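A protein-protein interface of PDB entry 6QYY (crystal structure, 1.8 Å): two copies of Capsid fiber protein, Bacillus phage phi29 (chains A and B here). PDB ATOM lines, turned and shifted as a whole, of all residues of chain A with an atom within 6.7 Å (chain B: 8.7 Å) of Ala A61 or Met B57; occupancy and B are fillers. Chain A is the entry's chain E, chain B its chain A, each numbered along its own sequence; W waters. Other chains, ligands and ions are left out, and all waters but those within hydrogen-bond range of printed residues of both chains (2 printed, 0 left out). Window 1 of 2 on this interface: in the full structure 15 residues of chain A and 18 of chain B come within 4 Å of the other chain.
The backbone NH (N) of Leu B60 lies within hydrogen-bond range of the backbone carbonyl oxygen (O) of Pro A59 (2.7 Å). O of Leu B60 lies within hydrogen-bond range of NZ of Lys A116.
The side-chain hydroxyl (OG) of Ser B4 lies close to the side-chain sulfur (SD) of Met B2 (3.6 Å). OD1 of Asn B56 is in hydrogen-bond range of OG of Ser B4 (2.7 Å). OH of Tyr B21 sits at hydrogen-bond distance from SD of Met B57 (3.3 Å). The backbone NH (N) of Ile B112 is in hydrogen-bond range of the backbone carbonyl oxygen (O) of Ala B61. The backbone NH (N) of Ile A112 is in hydrogen-bond range of the backbone carbonyl oxygen (O) of Ala A61 (2.9 Å). The backbone carbonyl oxygen (O) of Thr A109 sits at hydrogen-bond distance from the backbone NH (N) of Val A99, 3.0 Å away.
CD2 of Leu A60 touches CA of Pro B59 (3.8 Å). Leu A60 touches Leu B60 (C to CD1, 3.8 Å). CD1 of Leu B60 touches N of Ala A61, at 3.7 Å. Met B57 touches Ala A62 (SD to CB, 3.8 Å). Phe B5 touches Val A99 (CG to CG2, 3.6 Å). Val B3 touches Thr A109 (CG1 to CG2, 3.5 Å). Val A111 touches Tyr B21 (CG2 to CE2, 3.8 Å). CG2 of Ile B112 touches CB of Lys A116, 3.9 Å away. CD1 of Leu A117 touches O of Asp B40, at 3.4 Å. CG2 of Ile B112 touches CD2 of Leu A117, 3.8 Å away.
Ala A61 touches just these residues of chain B: Met B57 (3.5 Å) and Leu B60 (3.7 Å). Met B57 touches two residues of chain A. Of the printed residues of chain B, Ala A62 touches Met B57. Of the printed residues of chain A, Pro B59 touches Pro A59 and Leu A60. Printed residues of chain A within 4 Å of Tyr B21: Val A111 (3.8 Å). Printed residues of chain A within 4 Å of Leu B60: Pro A59 (2.7 Å), Leu A60 (3.8 Å), Ala A61 (3.7 Å) and Lys A116 (3.1 Å). Of the printed residues of chain A, Ser B4 touches Thr A109 (3.8 Å). The nearest residue of chain A that does not touch Met B57 is Val A111 (4.5 Å). The nearest printed residue of chain B that does not touch Val A99 is Tyr B21 (4.8 Å).
Of the 23 printed residues of chain B, 11 touch a printed residue of chain A. Hydrophobic or aromatic side chains of chain A within 4 Å of the printed part of chain B: Pro A59, Leu A60, Ala A61, Ala A62, Val A99, Val A111 and Leu A117. Among the printed residues, 17 pairs touch across the chains. Among the printed residues, no Asp or Glu carboxylate lies within 4 Å of a Lys or Arg side-chain nitrogen of the other chain.
Pro B59 touches its own counterpart, Pro A59. Pro A59 touches Leu B60, and with the chains exchanged Leu A60 touches Pro B59. Leu B60 touches its own counterpart, Leu A60. Ala A61 touches Leu B60, but with the chains exchanged Leu A60 does not touch Ala B61 (7.8 Å). Positions printed for both chains: 59, 60, 61, 63 and 112. Of the 17 pairs that touch across the chains among the printed residues, 4 have their exchanged pair printed and touching as well.
Water W2 lies within hydrogen-bond range of O of Ile B112 (2.7 Å), O of Ala B61 (2.8 Å) and NZ of Lys A116 (3.2 Å). Water W1 bridges the backbone NH of Ala A61 and the backbone carbonyl oxygen of Tyr B58.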
ATOM      1  N   PRO A  59      -2.043  35.798 -19.066  1.00  0.00           N
ATOM      2  CA  PRO A  59      -2.843  34.644 -19.492  1.00  0.00           C
ATOM      3  C   PRO A  59      -2.158  33.369 -19.017  1.00  0.00           C
ATOM      4  O   PRO A  59      -1.069  33.025 -19.480  1.00  0.00           O
ATOM      5  CB  PRO A  59      -2.835  34.768 -21.021  1.00  0.00           C
ATOM      6  CG  PRO A  59      -1.483  35.390 -21.318  1.00  0.00           C
ATOM      7  CD  PRO A  59      -1.139  36.274 -20.132  1.00  0.00           C
ATOM      8  N   LEU A  60      -2.760  32.714 -18.039  1.00  0.00           N
ATOM      9  CA  LEU A  60      -2.154  31.574 -17.358  1.00  0.00           C
ATOM     10  C   LEU A  60      -3.023  30.343 -17.509  1.00  0.00           C
ATOM     11  O   LEU A  60      -4.250  30.441 -17.608  1.00  0.00           O
ATOM     12  CB  LEU A  60      -1.983  31.843 -15.873  1.00  0.00           C
ATOM     13  CG  LEU A  60      -1.108  33.052 -15.551  1.00  0.00           C
ATOM     14  CD1 LEU A  60      -1.338  33.422 -14.097  1.00  0.00           C
ATOM     15  CD2 LEU A  60       0.347  32.756 -15.845  1.00  0.00           C
ATOM     16  N   ALA A  61      -2.377  29.183 -17.519  1.00  0.00           N
ATOM     17  CA  ALA A  61      -3.107  27.935 -17.430  1.00  0.00           C
ATOM     18  C   ALA A  61      -3.178  27.416 -15.999  1.00  0.00           C
ATOM     19  O   ALA A  61      -3.946  26.487 -15.729  1.00  0.00           O
ATOM     20  CB  ALA A  61      -2.481  26.885 -18.369  1.00  0.00           C
ATOM     21  N   ALA A  62      -2.423  28.010 -15.073  1.00  0.00           N
ATOM     22  CA  ALA A  62      -2.437  27.589 -13.682  1.00  0.00           C
ATOM     23  C   ALA A  62      -2.338  28.805 -12.777  1.00  0.00           C
ATOM     24  O   ALA A  62      -1.572  29.736 -13.048  1.00  0.00           O
ATOM     25  CB  ALA A  62      -1.287  26.629 -13.358  1.00  0.00           C
ATOM     26  N   TRP A  63      -3.096  28.758 -11.695  1.00  0.00           N
ATOM     27  CA  TRP A  63      -3.141  29.790 -10.675  1.00  0.00           C
ATOM     28  C   TRP A  63      -2.696  29.224  -9.331  1.00  0.00           C
ATOM     29  O   TRP A  63      -2.694  28.007  -9.122  1.00  0.00           O
ATOM     30  CB  TRP A  63      -4.563  30.339 -10.527  1.00  0.00           C
ATOM     31  CG  TRP A  63      -5.043  31.195 -11.671  1.00  0.00           C
ATOM     32  CD1 TRP A  63      -4.355  31.571 -12.802  1.00  0.00           C
ATOM     33  CD2 TRP A  63      -6.330  31.808 -11.760  1.00  0.00           C
ATOM     34  NE1 TRP A  63      -5.165  32.379 -13.598  1.00  0.00           N
ATOM     35  CE2 TRP A  63      -6.380  32.521 -12.977  1.00  0.00           C
ATOM     36  CE3 TRP A  63      -7.451  31.812 -10.928  1.00  0.00           C
ATOM     37  CZ2 TRP A  63      -7.510  33.239 -13.371  1.00  0.00           C
ATOM     38  CZ3 TRP A  63      -8.573  32.521 -11.324  1.00  0.00           C
ATOM     39  CH2 TRP A  63      -8.588  33.230 -12.528  1.00  0.00           C
ATOM     40  N   VAL A  99      -3.959  20.702  -8.455  1.00  0.00           N
ATOM     41  CA  VAL A  99      -2.878  19.807  -8.853  1.00  0.00           C
ATOM     42  C   VAL A  99      -1.953  19.494  -7.692  1.00  0.00           C
ATOM     43  O   VAL A  99      -0.890  18.896  -7.893  1.00  0.00           O
ATOM     44  CB  VAL A  99      -2.087  20.340 -10.055  1.00  0.00           C
ATOM     45  CG1 VAL A  99      -2.983  20.325 -11.294  1.00  0.00           C
ATOM     46  CG2 VAL A  99      -1.468  21.720  -9.757  1.00  0.00           C
ATOM     47  N   THR A 109      -2.069  25.133  -5.751  1.00  0.00           N
ATOM     48  CA  THR A 109      -1.886  25.333  -7.170  1.00  0.00           C
ATOM     49  C   THR A 109      -3.004  24.613  -7.900  1.00  0.00           C
ATOM     50  O   THR A 109      -3.393  23.502  -7.523  1.00  0.00           O
ATOM     51  CB  THR A 109      -0.519  24.820  -7.610  1.00  0.00           C
ATOM     52  OG1 THR A 109       0.482  25.468  -6.814  1.00  0.00           O
ATOM     53  CG2 THR A 109      -0.281  25.093  -9.062  1.00  0.00           C
ATOM     54  N   LEU A 110      -3.560  25.269  -8.910  1.00  0.00           N
ATOM     55  CA  LEU A 110      -4.696  24.702  -9.624  1.00  0.00           C
ATOM     56  C   LEU A 110      -4.571  25.027 -11.104  1.00  0.00           C
ATOM     57  O   LEU A 110      -3.927  26.001 -11.488  1.00  0.00           O
ATOM     58  CB  LEU A 110      -6.018  25.228  -9.072  1.00  0.00           C
ATOM     59  CG  LEU A 110      -6.181  26.746  -9.196  1.00  0.00           C
ATOM     60  CD1 LEU A 110      -7.044  27.052 -10.391  1.00  0.00           C
ATOM     61  CD2 LEU A 110      -6.827  27.321  -7.943  1.00  0.00           C
ATOM     62  N   VAL A 111      -5.175  24.180 -11.931  1.00  0.00           N
ATOM     63  CA  VAL A 111      -5.167  24.339 -13.384  1.00  0.00           C
ATOM     64  C   VAL A 111      -6.543  24.841 -13.811  1.00  0.00           C
ATOM     65  O   VAL A 111      -7.568  24.252 -13.449  1.00  0.00           O
ATOM     66  CB  VAL A 111      -4.787  23.013 -14.074  1.00  0.00           C
ATOM     67  CG1 VAL A 111      -5.127  23.055 -15.558  1.00  0.00           C
ATOM     68  CG2 VAL A 111      -3.299  22.723 -13.864  1.00  0.00           C
ATOM     69  N   ILE A 112      -6.564  25.942 -14.584  1.00  0.00           N
ATOM     70  CA  ILE A 112      -7.773  26.651 -14.991  1.00  0.00           C
ATOM     71  C   ILE A 112      -8.477  25.918 -16.132  1.00  0.00           C
ATOM     72  O   ILE A 112      -7.834  25.297 -16.983  1.00  0.00           O
ATOM     73  CB  ILE A 112      -7.382  28.087 -15.417  1.00  0.00           C
ATOM     74  CG1 ILE A 112      -6.889  28.879 -14.219  1.00  0.00           C
ATOM     75  CG2 ILE A 112      -8.540  28.823 -16.036  1.00  0.00           C
ATOM     76  CD1 ILE A 112      -7.936  29.080 -13.195  1.00  0.00           C
ATOM     77  N   SER A 113      -9.819  26.012 -16.159  1.00  0.00           N
ATOM     78  CA  SER A 113     -10.601  25.648 -17.344  1.00  0.00           C
ATOM     79  C   SER A 113     -10.596  26.757 -18.407  1.00  0.00           C
ATOM     80  O   SER A 113     -10.343  26.494 -19.590  1.00  0.00           O
ATOM     81  CB  SER A 113     -12.045  25.318 -16.948  1.00  0.00           C
ATOM     82  OG  SER A 113     -12.088  24.455 -15.823  1.00  0.00           O
ATOM     83  N   SER A 115      -8.881  29.141 -19.924  1.00  0.00           N
ATOM     84  CA  SER A 115      -7.650  29.743 -20.423  1.00  0.00           C
ATOM     85  C   SER A 115      -7.721  29.855 -21.951  1.00  0.00           C
ATOM     86  O   SER A 115      -8.785  29.672 -22.560  1.00  0.00           O
ATOM     87  CB  SER A 115      -6.430  28.928 -19.965  1.00  0.00           C
ATOM     88  OG  SER A 115      -6.476  27.596 -20.457  1.00  0.00           O
ATOM     89  N   LYS A 116      -6.576  30.162 -22.575  1.00  0.00           N
ATOM     90  CA  LYS A 116      -6.479  30.111 -24.033  1.00  0.00           C
ATOM     91  C   LYS A 116      -6.637  28.692 -24.573  1.00  0.00           C
ATOM     92  O   LYS A 116      -6.755  28.515 -25.794  1.00  0.00           O
ATOM     93  CB  LYS A 116      -5.137  30.694 -24.507  1.00  0.00           C
ATOM     94  CG  LYS A 116      -5.010  32.211 -24.400  1.00  0.00           C
ATOM     95  CD  LYS A 116      -3.742  32.703 -25.099  1.00  0.00           C
ATOM     96  CE  LYS A 116      -3.534  34.205 -24.928  1.00  0.00           C
ATOM     97  NZ  LYS A 116      -2.149  34.635 -25.324  1.00  0.00           N
ATOM     98  N   LEU A 117      -6.633  27.683 -23.699  1.00  0.00           N
ATOM     99  CA  LEU A 117      -6.769  26.285 -24.087  1.00  0.00           C
ATOM    100  C   LEU A 117      -8.209  25.777 -24.052  1.00  0.00           C
ATOM    101  O   LEU A 117      -8.469  24.674 -24.545  1.00  0.00           O
ATOM    102  CB  LEU A 117      -5.891  25.417 -23.180  1.00  0.00           C
ATOM    103  CG  LEU A 117      -4.401  25.589 -23.490  1.00  0.00           C
ATOM    104  CD1 LEU A 117      -3.491  24.928 -22.444  1.00  0.00           C
ATOM    105  CD2 LEU A 117      -4.112  25.037 -24.880  1.00  0.00           C
ATOM    106  N   MET B   1       7.049  35.072 -13.788  1.00  0.00           N
ATOM    107  CA  MET B   1       5.714  34.648 -13.389  1.00  0.00           C
ATOM    108  C   MET B   1       5.578  33.153 -13.659  1.00  0.00           C
ATOM    109  O   MET B   1       4.896  32.735 -14.589  1.00  0.00           O
ATOM    110  CB  MET B   1       4.642  35.450 -14.140  1.00  0.00           C
ATOM    111  CG  MET B   1       3.197  35.131 -13.751  1.00  0.00           C
ATOM    112  SD  MET B   1       2.891  35.041 -11.971  1.00  0.00           S
ATOM    113  CE  MET B   1       3.020  36.766 -11.495  1.00  0.00           C
ATOM    114  N   MET B   2       6.266  32.353 -12.858  1.00  0.00           N
ATOM    115  CA  MET B   2       6.238  30.905 -12.987  1.00  0.00           C
ATOM    116  C   MET B   2       5.428  30.312 -11.844  1.00  0.00           C
ATOM    117  O   MET B   2       5.454  30.818 -10.719  1.00  0.00           O
ATOM    118  CB  MET B   2       7.653  30.323 -12.989  1.00  0.00           C
ATOM    119  CG  MET B   2       7.722  28.832 -12.685  1.00  0.00           C
ATOM    120  SD  MET B   2       9.406  28.268 -12.397  1.00  0.00           S
ATOM    121  CE  MET B   2       9.565  28.485 -10.623  1.00  0.00           C
ATOM    122  N   VAL B   3       4.698  29.242 -12.146  1.00  0.00           N
ATOM    123  CA  VAL B   3       3.938  28.484 -11.161  1.00  0.00           C
ATOM    124  C   VAL B   3       4.368  27.027 -11.293  1.00  0.00           C
ATOM    125  O   VAL B   3       4.415  26.496 -12.409  1.00  0.00           O
ATOM    126  CB  VAL B   3       2.420  28.646 -11.384  1.00  0.00           C
ATOM    127  CG1 VAL B   3       1.642  27.586 -10.640  1.00  0.00           C
ATOM    128  CG2 VAL B   3       1.957  30.048 -10.977  1.00  0.00           C
ATOM    129  N   SER B   4       4.718  26.388 -10.171  1.00  0.00           N
ATOM    130  CA  SER B   4       5.272  25.039 -10.214  1.00  0.00           C
ATOM    131  C   SER B   4       4.477  24.090  -9.326  1.00  0.00           C
ATOM    132  O   SER B   4       3.891  24.503  -8.316  1.00  0.00           O
ATOM    133  CB  SER B   4       6.732  25.002  -9.771  1.00  0.00           C
ATOM    134  OG  SER B   4       7.456  26.068 -10.346  1.00  0.00           O
ATOM    135  N   PHE B   5       4.488  22.809  -9.711  1.00  0.00           N
ATOM    136  CA  PHE B   5       3.917  21.732  -8.915  1.00  0.00           C
ATOM    137  C   PHE B   5       4.636  20.432  -9.253  1.00  0.00           C
ATOM    138  O   PHE B   5       5.293  20.305 -10.292  1.00  0.00           O
ATOM    139  CB  PHE B   5       2.397  21.607  -9.123  1.00  0.00           C
ATOM    140  CG  PHE B   5       1.974  21.089 -10.491  1.00  0.00           C
ATOM    141  CD1 PHE B   5       1.704  19.737 -10.683  1.00  0.00           C
ATOM    142  CD2 PHE B   5       1.776  21.963 -11.556  1.00  0.00           C
ATOM    143  CE1 PHE B   5       1.288  19.260 -11.922  1.00  0.00           C
ATOM    144  CE2 PHE B   5       1.366  21.496 -12.801  1.00  0.00           C
ATOM    145  CZ  PHE B   5       1.125  20.140 -12.988  1.00  0.00           C
ATOM    146  N   LEU B  19       1.497  17.568 -23.272  1.00  0.00           N
ATOM    147  CA  LEU B  19       1.200  16.805 -22.066  1.00  0.00           C
ATOM    148  C   LEU B  19      -0.285  16.831 -21.718  1.00  0.00           C
ATOM    149  O   LEU B  19      -0.993  17.822 -21.959  1.00  0.00           O
ATOM    150  CB  LEU B  19       1.969  17.340 -20.857  1.00  0.00           C
ATOM    151  CG  LEU B  19       3.490  17.325 -20.884  1.00  0.00           C
ATOM    152  CD1 LEU B  19       4.018  18.047 -19.631  1.00  0.00           C
ATOM    153  CD2 LEU B  19       3.996  15.883 -20.972  1.00  0.00           C
ATOM    154  N   TYR B  21      -2.614  16.095 -18.202  1.00  0.00           N
ATOM    155  CA  TYR B  21      -2.610  15.874 -16.767  1.00  0.00           C
ATOM    156  C   TYR B  21      -3.685  14.856 -16.419  1.00  0.00           C
ATOM    157  O   TYR B  21      -4.786  14.888 -16.976  1.00  0.00           O
ATOM    158  CB  TYR B  21      -2.866  17.177 -16.020  1.00  0.00           C
ATOM    159  CG  TYR B  21      -1.817  18.230 -16.219  1.00  0.00           C
ATOM    160  CD1 TYR B  21      -0.546  17.904 -16.680  1.00  0.00           C
ATOM    161  CD2 TYR B  21      -2.102  19.568 -15.954  1.00  0.00           C
ATOM    162  CE1 TYR B  21       0.436  18.900 -16.842  1.00  0.00           C
ATOM    163  CE2 TYR B  21      -1.136  20.548 -16.103  1.00  0.00           C
ATOM    164  CZ  TYR B  21       0.119  20.219 -16.550  1.00  0.00           C
ATOM    165  OH  TYR B  21       1.060  21.213 -16.691  1.00  0.00           O
ATOM    166  N   ILE B  30       1.529  12.925 -15.326  1.00  0.00           N
ATOM    167  CA  ILE B  30       1.665  13.489 -16.659  1.00  0.00           C
ATOM    168  C   ILE B  30       2.002  12.369 -17.632  1.00  0.00           C
ATOM    169  O   ILE B  30       2.584  11.338 -17.268  1.00  0.00           O
ATOM    170  CB  ILE B  30       2.739  14.597 -16.722  1.00  0.00           C
ATOM    171  CG1 ILE B  30       4.092  14.050 -16.288  1.00  0.00           C
ATOM    172  CG2 ILE B  30       2.335  15.825 -15.881  1.00  0.00           C
ATOM    173  CD1 ILE B  30       5.256  15.018 -16.582  1.00  0.00           C
ATOM    174  N   PRO B  39      -4.175  19.483 -25.631  1.00  0.00           N
ATOM    175  CA  PRO B  39      -3.233  19.235 -24.541  1.00  0.00           C
ATOM    176  C   PRO B  39      -3.522  20.128 -23.349  1.00  0.00           C
ATOM    177  O   PRO B  39      -4.151  21.186 -23.457  1.00  0.00           O
ATOM    178  CB  PRO B  39      -1.874  19.578 -25.163  1.00  0.00           C
ATOM    179  CG  PRO B  39      -2.197  20.608 -26.190  1.00  0.00           C
ATOM    180  CD  PRO B  39      -3.540  20.176 -26.765  1.00  0.00           C
ATOM    181  N   ASP B  40      -3.050  19.678 -22.190  1.00  0.00           N
ATOM    182  CA  ASP B  40      -3.111  20.487 -20.977  1.00  0.00           C
ATOM    183  C   ASP B  40      -1.903  21.408 -20.848  1.00  0.00           C
ATOM    184  O   ASP B  40      -2.043  22.560 -20.417  1.00  0.00           O
ATOM    185  CB  ASP B  40      -3.217  19.584 -19.746  1.00  0.00           C
ATOM    186  CG  ASP B  40      -4.506  18.780 -19.723  1.00  0.00           C
ATOM    187  OD1 ASP B  40      -5.577  19.344 -20.074  1.00  0.00           O
ATOM    188  OD2 ASP B  40      -4.461  17.581 -19.359  1.00  0.00           O
ATOM    189  N   TYR B  41      -0.720  20.930 -21.219  1.00  0.00           N
ATOM    190  CA  TYR B  41       0.479  21.758 -21.180  1.00  0.00           C
ATOM    191  C   TYR B  41       1.512  21.118 -22.107  1.00  0.00           C
ATOM    192  O   TYR B  41       1.156  20.328 -22.988  1.00  0.00           O
ATOM    193  CB  TYR B  41       0.974  21.953 -19.731  1.00  0.00           C
ATOM    194  CG  TYR B  41       1.828  23.223 -19.607  1.00  0.00           C
ATOM    195  CD1 TYR B  41       1.297  24.469 -19.947  1.00  0.00           C
ATOM    196  CD2 TYR B  41       3.159  23.166 -19.204  1.00  0.00           C
ATOM    197  CE1 TYR B  41       2.078  25.631 -19.877  1.00  0.00           C
ATOM    198  CE2 TYR B  41       3.947  24.321 -19.131  1.00  0.00           C
ATOM    199  CZ  TYR B  41       3.399  25.548 -19.472  1.00  0.00           C
ATOM    200  OH  TYR B  41       4.171  26.697 -19.400  1.00  0.00           O
ATOM    201  N   VAL B  42       2.786  21.472 -21.923  1.00  0.00           N
ATOM    202  CA  VAL B  42       3.879  21.027 -22.777  1.00  0.00           C
ATOM    203  C   VAL B  42       5.101  20.755 -21.903  1.00  0.00           C
ATOM    204  O   VAL B  42       5.336  21.431 -20.896  1.00  0.00           O
ATOM    205  CB  VAL B  42       4.196  22.063 -23.882  1.00  0.00           C
ATOM    206  CG1 VAL B  42       4.620  23.405 -23.264  1.00  0.00           C
ATOM    207  CG2 VAL B  42       5.256  21.540 -24.847  1.00  0.00           C
ATOM    208  N   VAL B  44       9.128  20.562 -21.102  1.00  0.00           N
ATOM    209  CA  VAL B  44      10.412  21.112 -21.516  1.00  0.00           C
ATOM    210  C   VAL B  44      11.574  20.257 -21.062  1.00  0.00           C
ATOM    211  O   VAL B  44      12.731  20.650 -21.250  1.00  0.00           O
ATOM    212  CB  VAL B  44      10.600  22.566 -21.050  1.00  0.00           C
ATOM    213  CG1 VAL B  44       9.490  23.432 -21.623  1.00  0.00           C
ATOM    214  CG2 VAL B  44      10.632  22.619 -19.528  1.00  0.00           C
ATOM    215  N   GLN B  54       9.275  18.232 -11.486  1.00  0.00           N
ATOM    216  CA  GLN B  54       8.698  19.535 -11.187  1.00  0.00           C
ATOM    217  C   GLN B  54       8.209  20.138 -12.496  1.00  0.00           C
ATOM    218  O   GLN B  54       9.003  20.347 -13.421  1.00  0.00           O
ATOM    219  CB  GLN B  54       9.714  20.446 -10.500  1.00  0.00           C
ATOM    220  CG  GLN B  54       9.214  21.865 -10.319  1.00  0.00           C
ATOM    221  CD  GLN B  54       9.691  22.498  -9.024  1.00  0.00           C
ATOM    222  OE1 GLN B  54       9.863  21.816  -8.008  1.00  0.00           O
ATOM    223  NE2 GLN B  54       9.902  23.814  -9.055  1.00  0.00           N
ATOM    224  N   VAL B  55       6.909  20.398 -12.573  1.00  0.00           N
ATOM    225  CA  VAL B  55       6.293  20.974 -13.767  1.00  0.00           C
ATOM    226  C   VAL B  55       6.220  22.481 -13.572  1.00  0.00           C
ATOM    227  O   VAL B  55       5.527  22.955 -12.672  1.00  0.00           O
ATOM    228  CB  VAL B  55       4.887  20.401 -14.005  1.00  0.00           C
ATOM    229  CG1 VAL B  55       4.278  21.026 -15.268  1.00  0.00           C
ATOM    230  CG2 VAL B  55       4.912  18.876 -14.093  1.00  0.00           C
ATOM    231  N   ASN B  56       6.916  23.240 -14.418  1.00  0.00           N
ATOM    232  CA  ASN B  56       6.928  24.692 -14.303  1.00  0.00           C
ATOM    233  C   ASN B  56       6.052  25.281 -15.401  1.00  0.00           C
ATOM    234  O   ASN B  56       6.344  25.119 -16.589  1.00  0.00           O
ATOM    235  CB  ASN B  56       8.354  25.238 -14.399  1.00  0.00           C
ATOM    236  CG  ASN B  56       9.259  24.687 -13.304  1.00  0.00           C
ATOM    237  OD1 ASN B  56       8.873  24.621 -12.136  1.00  0.00           O
ATOM    238  ND2 ASN B  56      10.456  24.272 -13.684  1.00  0.00           N
ATOM    239  N   MET B  57       4.981  25.961 -15.012  1.00  0.00           N
ATOM    240  CA  MET B  57       4.077  26.523 -15.993  1.00  0.00           C
ATOM    241  C   MET B  57       4.242  28.037 -16.056  1.00  0.00           C
ATOM    242  O   MET B  57       4.387  28.707 -15.026  1.00  0.00           O
ATOM    243  CB  MET B  57       2.616  26.123 -15.722  1.00  0.00           C
ATOM    244  CG  MET B  57       2.350  24.633 -15.876  1.00  0.00           C
ATOM    245  SD  MET B  57       0.748  24.142 -15.304  1.00  0.00           S
ATOM    246  CE  MET B  57      -0.174  24.889 -16.650  1.00  0.00           C
ATOM    247  N   TYR B  58       4.252  28.547 -17.284  1.00  0.00           N
ATOM    248  CA  TYR B  58       4.544  29.923 -17.656  1.00  0.00           C
ATOM    249  C   TYR B  58       3.352  30.551 -18.368  1.00  0.00           C
ATOM    250  O   TYR B  58       2.471  29.838 -18.862  1.00  0.00           O
ATOM    251  CB  TYR B  58       5.771  29.962 -18.582  1.00  0.00           C
ATOM    252  CG  TYR B  58       7.051  29.693 -17.825  1.00  0.00           C
ATOM    253  CD1 TYR B  58       7.695  30.719 -17.148  1.00  0.00           C
ATOM    254  CD2 TYR B  58       7.589  28.409 -17.750  1.00  0.00           C
ATOM    255  CE1 TYR B  58       8.861  30.492 -16.425  1.00  0.00           C
ATOM    256  CE2 TYR B  58       8.772  28.166 -17.025  1.00  0.00           C
ATOM    257  CZ  TYR B  58       9.394  29.219 -16.368  1.00  0.00           C
ATOM    258  OH  TYR B  58      10.557  29.023 -15.644  1.00  0.00           O
ATOM    259  N   PRO B  59       3.289  31.886 -18.432  1.00  0.00           N
ATOM    260  CA  PRO B  59       2.203  32.546 -19.172  1.00  0.00           C
ATOM    261  C   PRO B  59       2.110  32.051 -20.608  1.00  0.00           C
ATOM    262  O   PRO B  59       3.112  31.716 -21.241  1.00  0.00           O
ATOM    263  CB  PRO B  59       2.585  34.033 -19.111  1.00  0.00           C
ATOM    264  CG  PRO B  59       3.353  34.157 -17.810  1.00  0.00           C
ATOM    265  CD  PRO B  59       4.145  32.856 -17.717  1.00  0.00           C
ATOM    266  N   LEU B  60       0.879  31.984 -21.106  1.00  0.00           N
ATOM    267  CA  LEU B  60       0.589  31.364 -22.395  1.00  0.00           C
ATOM    268  C   LEU B  60       0.703  32.381 -23.524  1.00  0.00           C
ATOM    269  O   LEU B  60      -0.005  33.397 -23.536  1.00  0.00           O
ATOM    270  CB  LEU B  60      -0.812  30.761 -22.389  1.00  0.00           C
ATOM    271  CG  LEU B  60      -1.110  29.779 -21.248  1.00  0.00           C
ATOM    272  CD1 LEU B  60      -2.616  29.513 -21.184  1.00  0.00           C
ATOM    273  CD2 LEU B  60      -0.326  28.482 -21.461  1.00  0.00           C
ATOM    274  N   ALA B  61       1.570  32.099 -24.483  1.00  0.00           N
ATOM    275  CA  ALA B  61       1.493  32.777 -25.768  1.00  0.00           C
ATOM    276  C   ALA B  61       1.920  31.790 -26.845  1.00  0.00           C
ATOM    277  O   ALA B  61       1.099  31.365 -27.664  1.00  0.00           O
ATOM    278  CB  ALA B  61       2.356  34.040 -25.793  1.00  0.00           C
ATOM    279  N   TRP B  63       4.295  28.100 -27.784  1.00  0.00           N
ATOM    280  CA  TRP B  63       4.955  26.881 -27.309  1.00  0.00           C
ATOM    281  C   TRP B  63       5.918  26.361 -28.364  1.00  0.00           C
ATOM    282  O   TRP B  63       5.705  26.551 -29.562  1.00  0.00           O
ATOM    283  CB  TRP B  63       3.959  25.765 -27.010  1.00  0.00           C
ATOM    284  CG  TRP B  63       3.222  25.878 -25.737  1.00  0.00           C
ATOM    285  CD1 TRP B  63       3.510  26.695 -24.673  1.00  0.00           C
ATOM    286  CD2 TRP B  63       2.062  25.137 -25.376  1.00  0.00           C
ATOM    287  NE1 TRP B  63       2.584  26.500 -23.673  1.00  0.00           N
ATOM    288  CE2 TRP B  63       1.679  25.557 -24.084  1.00  0.00           C
ATOM    289  CE3 TRP B  63       1.289  24.167 -26.029  1.00  0.00           C
ATOM    290  CZ2 TRP B  63       0.560  25.027 -23.426  1.00  0.00           C
ATOM    291  CZ3 TRP B  63       0.182  23.635 -25.369  1.00  0.00           C
ATOM    292  CH2 TRP B  63      -0.176  24.075 -24.090  1.00  0.00           C
ATOM    293  N   ILE B 112      -0.657  29.626 -29.254  1.00  0.00           N
ATOM    294  CA  ILE B 112      -1.799  28.939 -28.660  1.00  0.00           C
ATOM    295  C   ILE B 112      -3.081  29.691 -29.000  1.00  0.00           C
ATOM    296  O   ILE B 112      -3.203  30.900 -28.752  1.00  0.00           O
ATOM    297  CB  ILE B 112      -1.614  28.814 -27.143  1.00  0.00           C
ATOM    298  CG1 ILE B 112      -0.374  27.984 -26.837  1.00  0.00           C
ATOM    299  CG2 ILE B 112      -2.856  28.210 -26.497  1.00  0.00           C
ATOM    300  CD1 ILE B 112       0.255  28.336 -25.476  1.00  0.00           C
HETATM  301  O   HOH W   1       0.298  28.803 -17.346  1.00  0.00           O
HETATM  302  O   HOH W   2      -1.424  32.632 -27.712  1.00  0.00           O
